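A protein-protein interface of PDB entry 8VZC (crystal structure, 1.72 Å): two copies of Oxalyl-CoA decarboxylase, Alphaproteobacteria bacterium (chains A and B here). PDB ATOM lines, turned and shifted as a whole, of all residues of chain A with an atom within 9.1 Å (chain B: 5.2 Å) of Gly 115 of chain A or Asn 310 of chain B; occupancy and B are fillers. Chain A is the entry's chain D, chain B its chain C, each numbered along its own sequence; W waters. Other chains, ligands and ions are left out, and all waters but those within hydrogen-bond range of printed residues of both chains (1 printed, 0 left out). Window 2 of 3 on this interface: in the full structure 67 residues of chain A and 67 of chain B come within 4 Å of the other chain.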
ATOM      1  N   SER A 109     -33.619  24.675  31.066  1.00  0.00           N
ATOM      2  CA  SER A 109     -32.424  25.499  30.985  1.00  0.00           C
ATOM      3  C   SER A 109     -32.732  26.772  30.194  1.00  0.00           C
ATOM      4  O   SER A 109     -33.708  26.841  29.431  1.00  0.00           O
ATOM      5  CB  SER A 109     -31.258  24.711  30.365  1.00  0.00           C
ATOM      6  OG  SER A 109     -31.586  24.157  29.089  1.00  0.00           O
ATOM      7  N   ALA A 110     -31.923  27.816  30.434  1.00  0.00           N
ATOM      8  CA  ALA A 110     -32.182  29.121  29.815  1.00  0.00           C
ATOM      9  C   ALA A 110     -32.138  29.049  28.290  1.00  0.00           C
ATOM     10  O   ALA A 110     -31.266  28.404  27.694  1.00  0.00           O
ATOM     11  CB  ALA A 110     -31.165  30.153  30.336  1.00  0.00           C
ATOM     12  N   ILE A 111     -33.099  29.734  27.636  1.00  0.00           N
ATOM     13  CA  ILE A 111     -33.144  29.697  26.181  1.00  0.00           C
ATOM     14  C   ILE A 111     -31.830  30.155  25.569  1.00  0.00           C
ATOM     15  O   ILE A 111     -31.392  29.620  24.551  1.00  0.00           O
ATOM     16  CB  ILE A 111     -34.317  30.551  25.642  1.00  0.00           C
ATOM     17  CG1 ILE A 111     -35.626  30.012  26.166  1.00  0.00           C
ATOM     18  CG2 ILE A 111     -34.300  30.500  24.110  1.00  0.00           C
ATOM     19  CD1 ILE A 111     -35.867  28.572  25.768  1.00  0.00           C
ATOM     20  N   GLU A 112     -31.207  31.189  26.140  1.00  0.00           N
ATOM     21  CA  GLU A 112     -30.010  31.729  25.506  1.00  0.00           C
ATOM     22  C   GLU A 112     -28.817  30.763  25.543  1.00  0.00           C
ATOM     23  O   GLU A 112     -27.848  30.989  24.812  1.00  0.00           O
ATOM     24  CB  GLU A 112     -29.637  33.068  26.157  1.00  0.00           C
ATOM     25  CG  GLU A 112     -29.219  32.955  27.621  1.00  0.00           C
ATOM     26  CD  GLU A 112     -28.485  34.199  28.113  1.00  0.00           C
ATOM     27  OE1 GLU A 112     -29.116  35.280  28.184  1.00  0.00           O
ATOM     28  OE2 GLU A 112     -27.270  34.100  28.406  1.00  0.00           O
ATOM     29  N   GLN A 113     -28.867  29.683  26.327  1.00  0.00           N
ATOM     30  CA  GLN A 113     -27.808  28.669  26.303  1.00  0.00           C
ATOM     31  C   GLN A 113     -28.141  27.452  25.439  1.00  0.00           C
ATOM     32  O   GLN A 113     -27.345  26.511  25.392  1.00  0.00           O
ATOM     33  CB  GLN A 113     -27.461  28.191  27.732  1.00  0.00           C
ATOM     34  CG  GLN A 113     -26.956  29.296  28.654  1.00  0.00           C
ATOM     35  CD  GLN A 113     -26.345  28.778  29.973  1.00  0.00           C
ATOM     36  OE1 GLN A 113     -26.895  27.899  30.635  1.00  0.00           O
ATOM     37  NE2 GLN A 113     -25.215  29.344  30.353  1.00  0.00           N
ATOM     38  N   ASN A 114     -29.271  27.440  24.729  1.00  0.00           N
ATOM     39  CA  ASN A 114     -29.622  26.263  23.940  1.00  0.00           C
ATOM     40  C   ASN A 114     -28.561  25.997  22.884  1.00  0.00           C
ATOM     41  O   ASN A 114     -27.994  26.929  22.318  1.00  0.00           O
ATOM     42  CB  ASN A 114     -30.987  26.453  23.251  1.00  0.00           C
ATOM     43  CG  ASN A 114     -32.167  26.258  24.206  1.00  0.00           C
ATOM     44  OD1 ASN A 114     -31.994  25.783  25.344  1.00  0.00           O
ATOM     45  ND2 ASN A 114     -33.395  26.599  23.731  1.00  0.00           N
ATOM     46  N   GLY A 115     -28.291  24.711  22.629  1.00  0.00           N
ATOM     47  CA  GLY A 115     -27.197  24.279  21.786  1.00  0.00           C
ATOM     48  C   GLY A 115     -25.854  24.102  22.494  1.00  0.00           C
ATOM     49  O   GLY A 115     -24.954  23.456  21.934  1.00  0.00           O
ATOM     50  N   MET A 116     -25.674  24.698  23.665  1.00  0.00           N
ATOM     51  CA  MET A 116     -24.328  24.774  24.252  1.00  0.00           C
ATOM     52  C   MET A 116     -23.994  23.620  25.175  1.00  0.00           C
ATOM     53  O   MET A 116     -22.829  23.519  25.620  1.00  0.00           O
ATOM     54  CB  MET A 116     -24.159  26.075  25.035  1.00  0.00           C
ATOM     55  CG  MET A 116     -24.229  27.314  24.206  1.00  0.00           C
ATOM     56  SD  MET A 116     -24.190  28.810  25.201  1.00  0.00           S
ATOM     57  CE  MET A 116     -22.538  28.744  25.887  1.00  0.00           C
ATOM     58  N   GLY A 117     -24.952  22.748  25.473  1.00  0.00           N
ATOM     59  CA  GLY A 117     -24.733  21.714  26.477  1.00  0.00           C
ATOM     60  C   GLY A 117     -24.916  22.281  27.866  1.00  0.00           C
ATOM     61  O   GLY A 117     -24.076  22.100  28.764  1.00  0.00           O
ATOM     62  N   ALA A 118     -26.002  23.030  28.032  1.00  0.00           N
ATOM     63  CA  ALA A 118     -26.299  23.676  29.304  1.00  0.00           C
ATOM     64  C   ALA A 118     -26.659  22.637  30.367  1.00  0.00           C
ATOM     65  O   ALA A 118     -27.069  21.513  30.057  1.00  0.00           O
ATOM     66  CB  ALA A 118     -27.455  24.682  29.139  1.00  0.00           C
ATOM     67  N   GLU A 121     -30.000  20.757  29.977  1.00  0.00           N
ATOM     68  CA  GLU A 121     -30.618  21.010  28.671  1.00  0.00           C
ATOM     69  C   GLU A 121     -31.263  19.730  28.152  1.00  0.00           C
ATOM     70  O   GLU A 121     -30.653  18.656  28.169  1.00  0.00           O
ATOM     71  CB  GLU A 121     -29.565  21.522  27.675  1.00  0.00           C
ATOM     72  CG  GLU A 121     -30.128  21.893  26.285  1.00  0.00           C
ATOM     73  CD  GLU A 121     -29.059  22.462  25.355  1.00  0.00           C
ATOM     74  OE1 GLU A 121     -27.888  22.636  25.787  1.00  0.00           O
ATOM     75  OE2 GLU A 121     -29.393  22.749  24.187  1.00  0.00           O
ATOM     76  N   GLU A 122     -32.509  19.833  27.688  1.00  0.00           N
ATOM     77  CA  GLU A 122     -33.178  18.625  27.243  1.00  0.00           C
ATOM     78  C   GLU A 122     -34.323  19.038  26.325  1.00  0.00           C
ATOM     79  O   GLU A 122     -34.854  20.148  26.449  1.00  0.00           O
ATOM     80  CB  GLU A 122     -33.722  17.815  28.435  1.00  0.00           C
ATOM     81  CG  GLU A 122     -34.408  16.476  28.079  1.00  0.00           C
ATOM     82  CD  GLU A 122     -33.489  15.553  27.277  1.00  0.00           C
ATOM     83  OE1 GLU A 122     -32.687  14.798  27.903  1.00  0.00           O
ATOM     84  OE2 GLU A 122     -33.539  15.613  26.023  1.00  0.00           O
ATOM     85  N   PHE B 280     -16.722  20.705  26.358  1.00  0.00           N
ATOM     86  CA  PHE B 280     -16.995  22.084  26.773  1.00  0.00           C
ATOM     87  C   PHE B 280     -18.507  22.278  26.945  1.00  0.00           C
ATOM     88  O   PHE B 280     -19.136  23.129  26.312  1.00  0.00           O
ATOM     89  CB  PHE B 280     -16.438  23.075  25.757  1.00  0.00           C
ATOM     90  CG  PHE B 280     -14.988  23.444  25.962  1.00  0.00           C
ATOM     91  CD1 PHE B 280     -14.402  23.404  27.223  1.00  0.00           C
ATOM     92  CD2 PHE B 280     -14.221  23.837  24.878  1.00  0.00           C
ATOM     93  CE1 PHE B 280     -13.072  23.773  27.380  1.00  0.00           C
ATOM     94  CE2 PHE B 280     -12.876  24.202  25.030  1.00  0.00           C
ATOM     95  CZ  PHE B 280     -12.317  24.157  26.281  1.00  0.00           C
ATOM     96  N   PHE B 286     -18.245  25.706  29.264  1.00  0.00           N
ATOM     97  CA  PHE B 286     -18.355  25.945  27.820  1.00  0.00           C
ATOM     98  C   PHE B 286     -17.060  26.344  27.127  1.00  0.00           C
ATOM     99  O   PHE B 286     -17.081  26.589  25.916  1.00  0.00           O
ATOM    100  CB  PHE B 286     -19.434  26.992  27.518  1.00  0.00           C
ATOM    101  CG  PHE B 286     -20.704  26.733  28.276  1.00  0.00           C
ATOM    102  CD1 PHE B 286     -21.503  25.634  27.956  1.00  0.00           C
ATOM    103  CD2 PHE B 286     -21.078  27.540  29.356  1.00  0.00           C
ATOM    104  CE1 PHE B 286     -22.703  25.385  28.688  1.00  0.00           C
ATOM    105  CE2 PHE B 286     -22.239  27.293  30.075  1.00  0.00           C
ATOM    106  CZ  PHE B 286     -23.065  26.215  29.741  1.00  0.00           C
ATOM    107  N   GLN B 300      -8.266  19.181  21.096  1.00  0.00           N
ATOM    108  CA  GLN B 300      -9.447  18.451  21.548  1.00  0.00           C
ATOM    109  C   GLN B 300      -9.395  17.016  21.066  1.00  0.00           C
ATOM    110  O   GLN B 300      -9.417  16.775  19.855  1.00  0.00           O
ATOM    111  CB  GLN B 300     -10.736  19.120  21.033  1.00  0.00           C
ATOM    112  CG  GLN B 300     -12.000  18.539  21.634  1.00  0.00           C
ATOM    113  CD  GLN B 300     -13.209  19.305  21.120  1.00  0.00           C
ATOM    114  OE1 GLN B 300     -13.046  20.268  20.374  1.00  0.00           O
ATOM    115  NE2 GLN B 300     -14.412  18.880  21.502  1.00  0.00           N
ATOM    116  N   GLU B 306     -18.378  15.210  15.567  1.00  0.00           N
ATOM    117  CA  GLU B 306     -19.335  16.319  15.662  1.00  0.00           C
ATOM    118  C   GLU B 306     -19.169  17.145  16.941  1.00  0.00           C
ATOM    119  O   GLU B 306     -19.618  18.289  16.982  1.00  0.00           O
ATOM    120  CB  GLU B 306     -20.760  15.791  15.571  1.00  0.00           C
ATOM    121  CG  GLU B 306     -21.054  15.069  14.263  1.00  0.00           C
ATOM    122  CD  GLU B 306     -20.878  13.556  14.349  1.00  0.00           C
ATOM    123  OE1 GLU B 306     -20.018  13.059  15.127  1.00  0.00           O
ATOM    124  OE2 GLU B 306     -21.609  12.855  13.623  1.00  0.00           O
ATOM    125  N   GLU B 307     -18.512  16.615  17.974  1.00  0.00           N
ATOM    126  CA  GLU B 307     -18.255  17.396  19.181  1.00  0.00           C
ATOM    127  C   GLU B 307     -17.133  18.430  18.996  1.00  0.00           C
ATOM    128  O   GLU B 307     -17.060  19.387  19.775  1.00  0.00           O
ATOM    129  CB  GLU B 307     -17.882  16.444  20.325  1.00  0.00           C
ATOM    130  CG  GLU B 307     -17.846  17.061  21.732  1.00  0.00           C
ATOM    131  CD  GLU B 307     -19.225  17.515  22.196  1.00  0.00           C
ATOM    132  OE1 GLU B 307     -20.222  16.817  21.895  1.00  0.00           O
ATOM    133  OE2 GLU B 307     -19.315  18.578  22.865  1.00  0.00           O
ATOM    134  N   ILE B 308     -16.263  18.262  17.990  1.00  0.00           N
ATOM    135  CA  ILE B 308     -15.061  19.091  17.861  1.00  0.00           C
ATOM    136  C   ILE B 308     -15.435  20.549  17.615  1.00  0.00           C
ATOM    137  O   ILE B 308     -16.175  20.870  16.675  1.00  0.00           O
ATOM    138  CB  ILE B 308     -14.177  18.562  16.719  1.00  0.00           C
ATOM    139  CG1 ILE B 308     -13.706  17.142  17.027  1.00  0.00           C
ATOM    140  CG2 ILE B 308     -12.990  19.510  16.479  1.00  0.00           C
ATOM    141  CD1 ILE B 308     -12.859  17.035  18.335  1.00  0.00           C
ATOM    142  N   GLY B 309     -14.896  21.448  18.434  1.00  0.00           N
ATOM    143  CA  GLY B 309     -15.145  22.860  18.244  1.00  0.00           C
ATOM    144  C   GLY B 309     -16.472  23.378  18.784  1.00  0.00           C
ATOM    145  O   GLY B 309     -16.786  24.554  18.573  1.00  0.00           O
ATOM    146  N   ASN B 310     -17.273  22.555  19.459  1.00  0.00           N
ATOM    147  CA  ASN B 310     -18.481  23.078  20.096  1.00  0.00           C
ATOM    148  C   ASN B 310     -18.145  24.216  21.068  1.00  0.00           C
ATOM    149  O   ASN B 310     -17.223  24.108  21.885  1.00  0.00           O
ATOM    150  CB  ASN B 310     -19.219  21.969  20.831  1.00  0.00           C
ATOM    151  CG  ASN B 310     -20.684  22.094  20.654  1.00  0.00           C
ATOM    152  OD1 ASN B 310     -21.143  22.109  19.516  1.00  0.00           O
ATOM    153  ND2 ASN B 310     -21.441  22.277  21.759  1.00  0.00           N
ATOM    154  N   ASN B 311     -18.884  25.317  20.947  1.00  0.00           N
ATOM    155  CA  ASN B 311     -18.748  26.527  21.765  1.00  0.00           C
ATOM    156  C   ASN B 311     -17.430  27.267  21.562  1.00  0.00           C
ATOM    157  O   ASN B 311     -17.443  28.490  21.382  1.00  0.00           O
ATOM    158  CB  ASN B 311     -18.920  26.212  23.254  1.00  0.00           C
ATOM    159  CG  ASN B 311     -20.307  25.733  23.573  1.00  0.00           C
ATOM    160  OD1 ASN B 311     -21.301  26.262  23.036  1.00  0.00           O
ATOM    161  ND2 ASN B 311     -20.405  24.743  24.439  1.00  0.00           N
ATOM    162  N   ARG B 312     -16.300  26.562  21.623  1.00  0.00           N
ATOM    163  CA  ARG B 312     -14.998  27.172  21.354  1.00  0.00           C
ATOM    164  C   ARG B 312     -14.262  26.375  20.282  1.00  0.00           C
ATOM    165  O   ARG B 312     -14.080  25.155  20.417  1.00  0.00           O
ATOM    166  CB  ARG B 312     -14.154  27.253  22.627  1.00  0.00           C
ATOM    167  CG  ARG B 312     -12.757  27.823  22.404  1.00  0.00           C
ATOM    168  CD  ARG B 312     -12.777  29.267  21.933  1.00  0.00           C
ATOM    169  NE  ARG B 312     -11.411  29.757  21.720  1.00  0.00           N
ATOM    170  CZ  ARG B 312     -11.071  30.720  20.875  1.00  0.00           C
ATOM    171  NH1 ARG B 312     -11.984  31.365  20.147  1.00  0.00           N
ATOM    172  NH2 ARG B 312      -9.787  31.027  20.722  1.00  0.00           N
HETATM  173  O   HOH W   1     -21.078  20.687  24.697  1.00  0.00           O
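Among the printed residues, merely in contact across the chains: Met 116 of chain A with Phe 286 of chain B (3.4 Å), Gly 117 of chain A with Phe 286 of chain B (3.6 Å), Gln 113 of chain A with Phe 286 of chain B (3.6 Å), Gly 115 of chain A with Asn 310 of chain B (3.7 Å) and Met 116 of chain A with Phe 280 of chain B (3.8 Å).
ND2 of Asn 311 of chain B sits at hydrogen-bond distance from O of Met 116 of chain A.
The backbone carbonyl oxygen (O) of Phe 280 of chain B sits at hydrogen-bond distance from the side-chain amide nitrogen (ND2) of Asn 311 of chain B (2.8 Å).
OE2 of Glu 121 of chain A sits at hydrogen-bond distance from N of Gly 115 of chain A (2.7 Å).
The backbone NH (N) of Gly 117 of chain A is in hydrogen-bond range of the side-chain carboxylate (OE1) of Glu 121 of chain A (3.0 Å).
No position is printed for both chains.
Of the 6 pairs that touch across the chains among the printed residues, none has its exchanged pair printed and touching as well.
Water W1 lies within hydrogen-bond range of the side-chain carboxylate of Glu 307 of chain B (3.3 Å), the side-chain amide nitrogen of Asn 310 of chain B (3.4 Å) and the backbone carbonyl oxygen of Met 116 of chain A (3.5 Å).
Gly 115 of chain A touches just one residue of chain B: Asn 310.
Asn 310 of chain B touches one residue of chain A.
Printed residues of chain A within 4 Å of Phe 280 of chain B: Met 116.
Printed residues of chain B within 4 Å of Gln 113 of chain A: Phe 286.
The nearest residue of chain A that does not touch Asn 310 of chain B is Met 116 of chain A (4.3 Å).
Of the 12 printed residues of chain A, 4 touch a printed residue of chain B.
Printed residues of chain A that touch a printed residue of chain B: Gln 113, Gly 115, Met 116 and Gly 117.
Hydrophobic or aromatic side chains of chain A within 4 Å of the printed part of chain B: Met 116.
Hydrophobic or aromatic side chains of chain B within 4 Å of the printed part of chain A: Phe 286.
Among the printed residues, 6 pairs touch across the chains.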
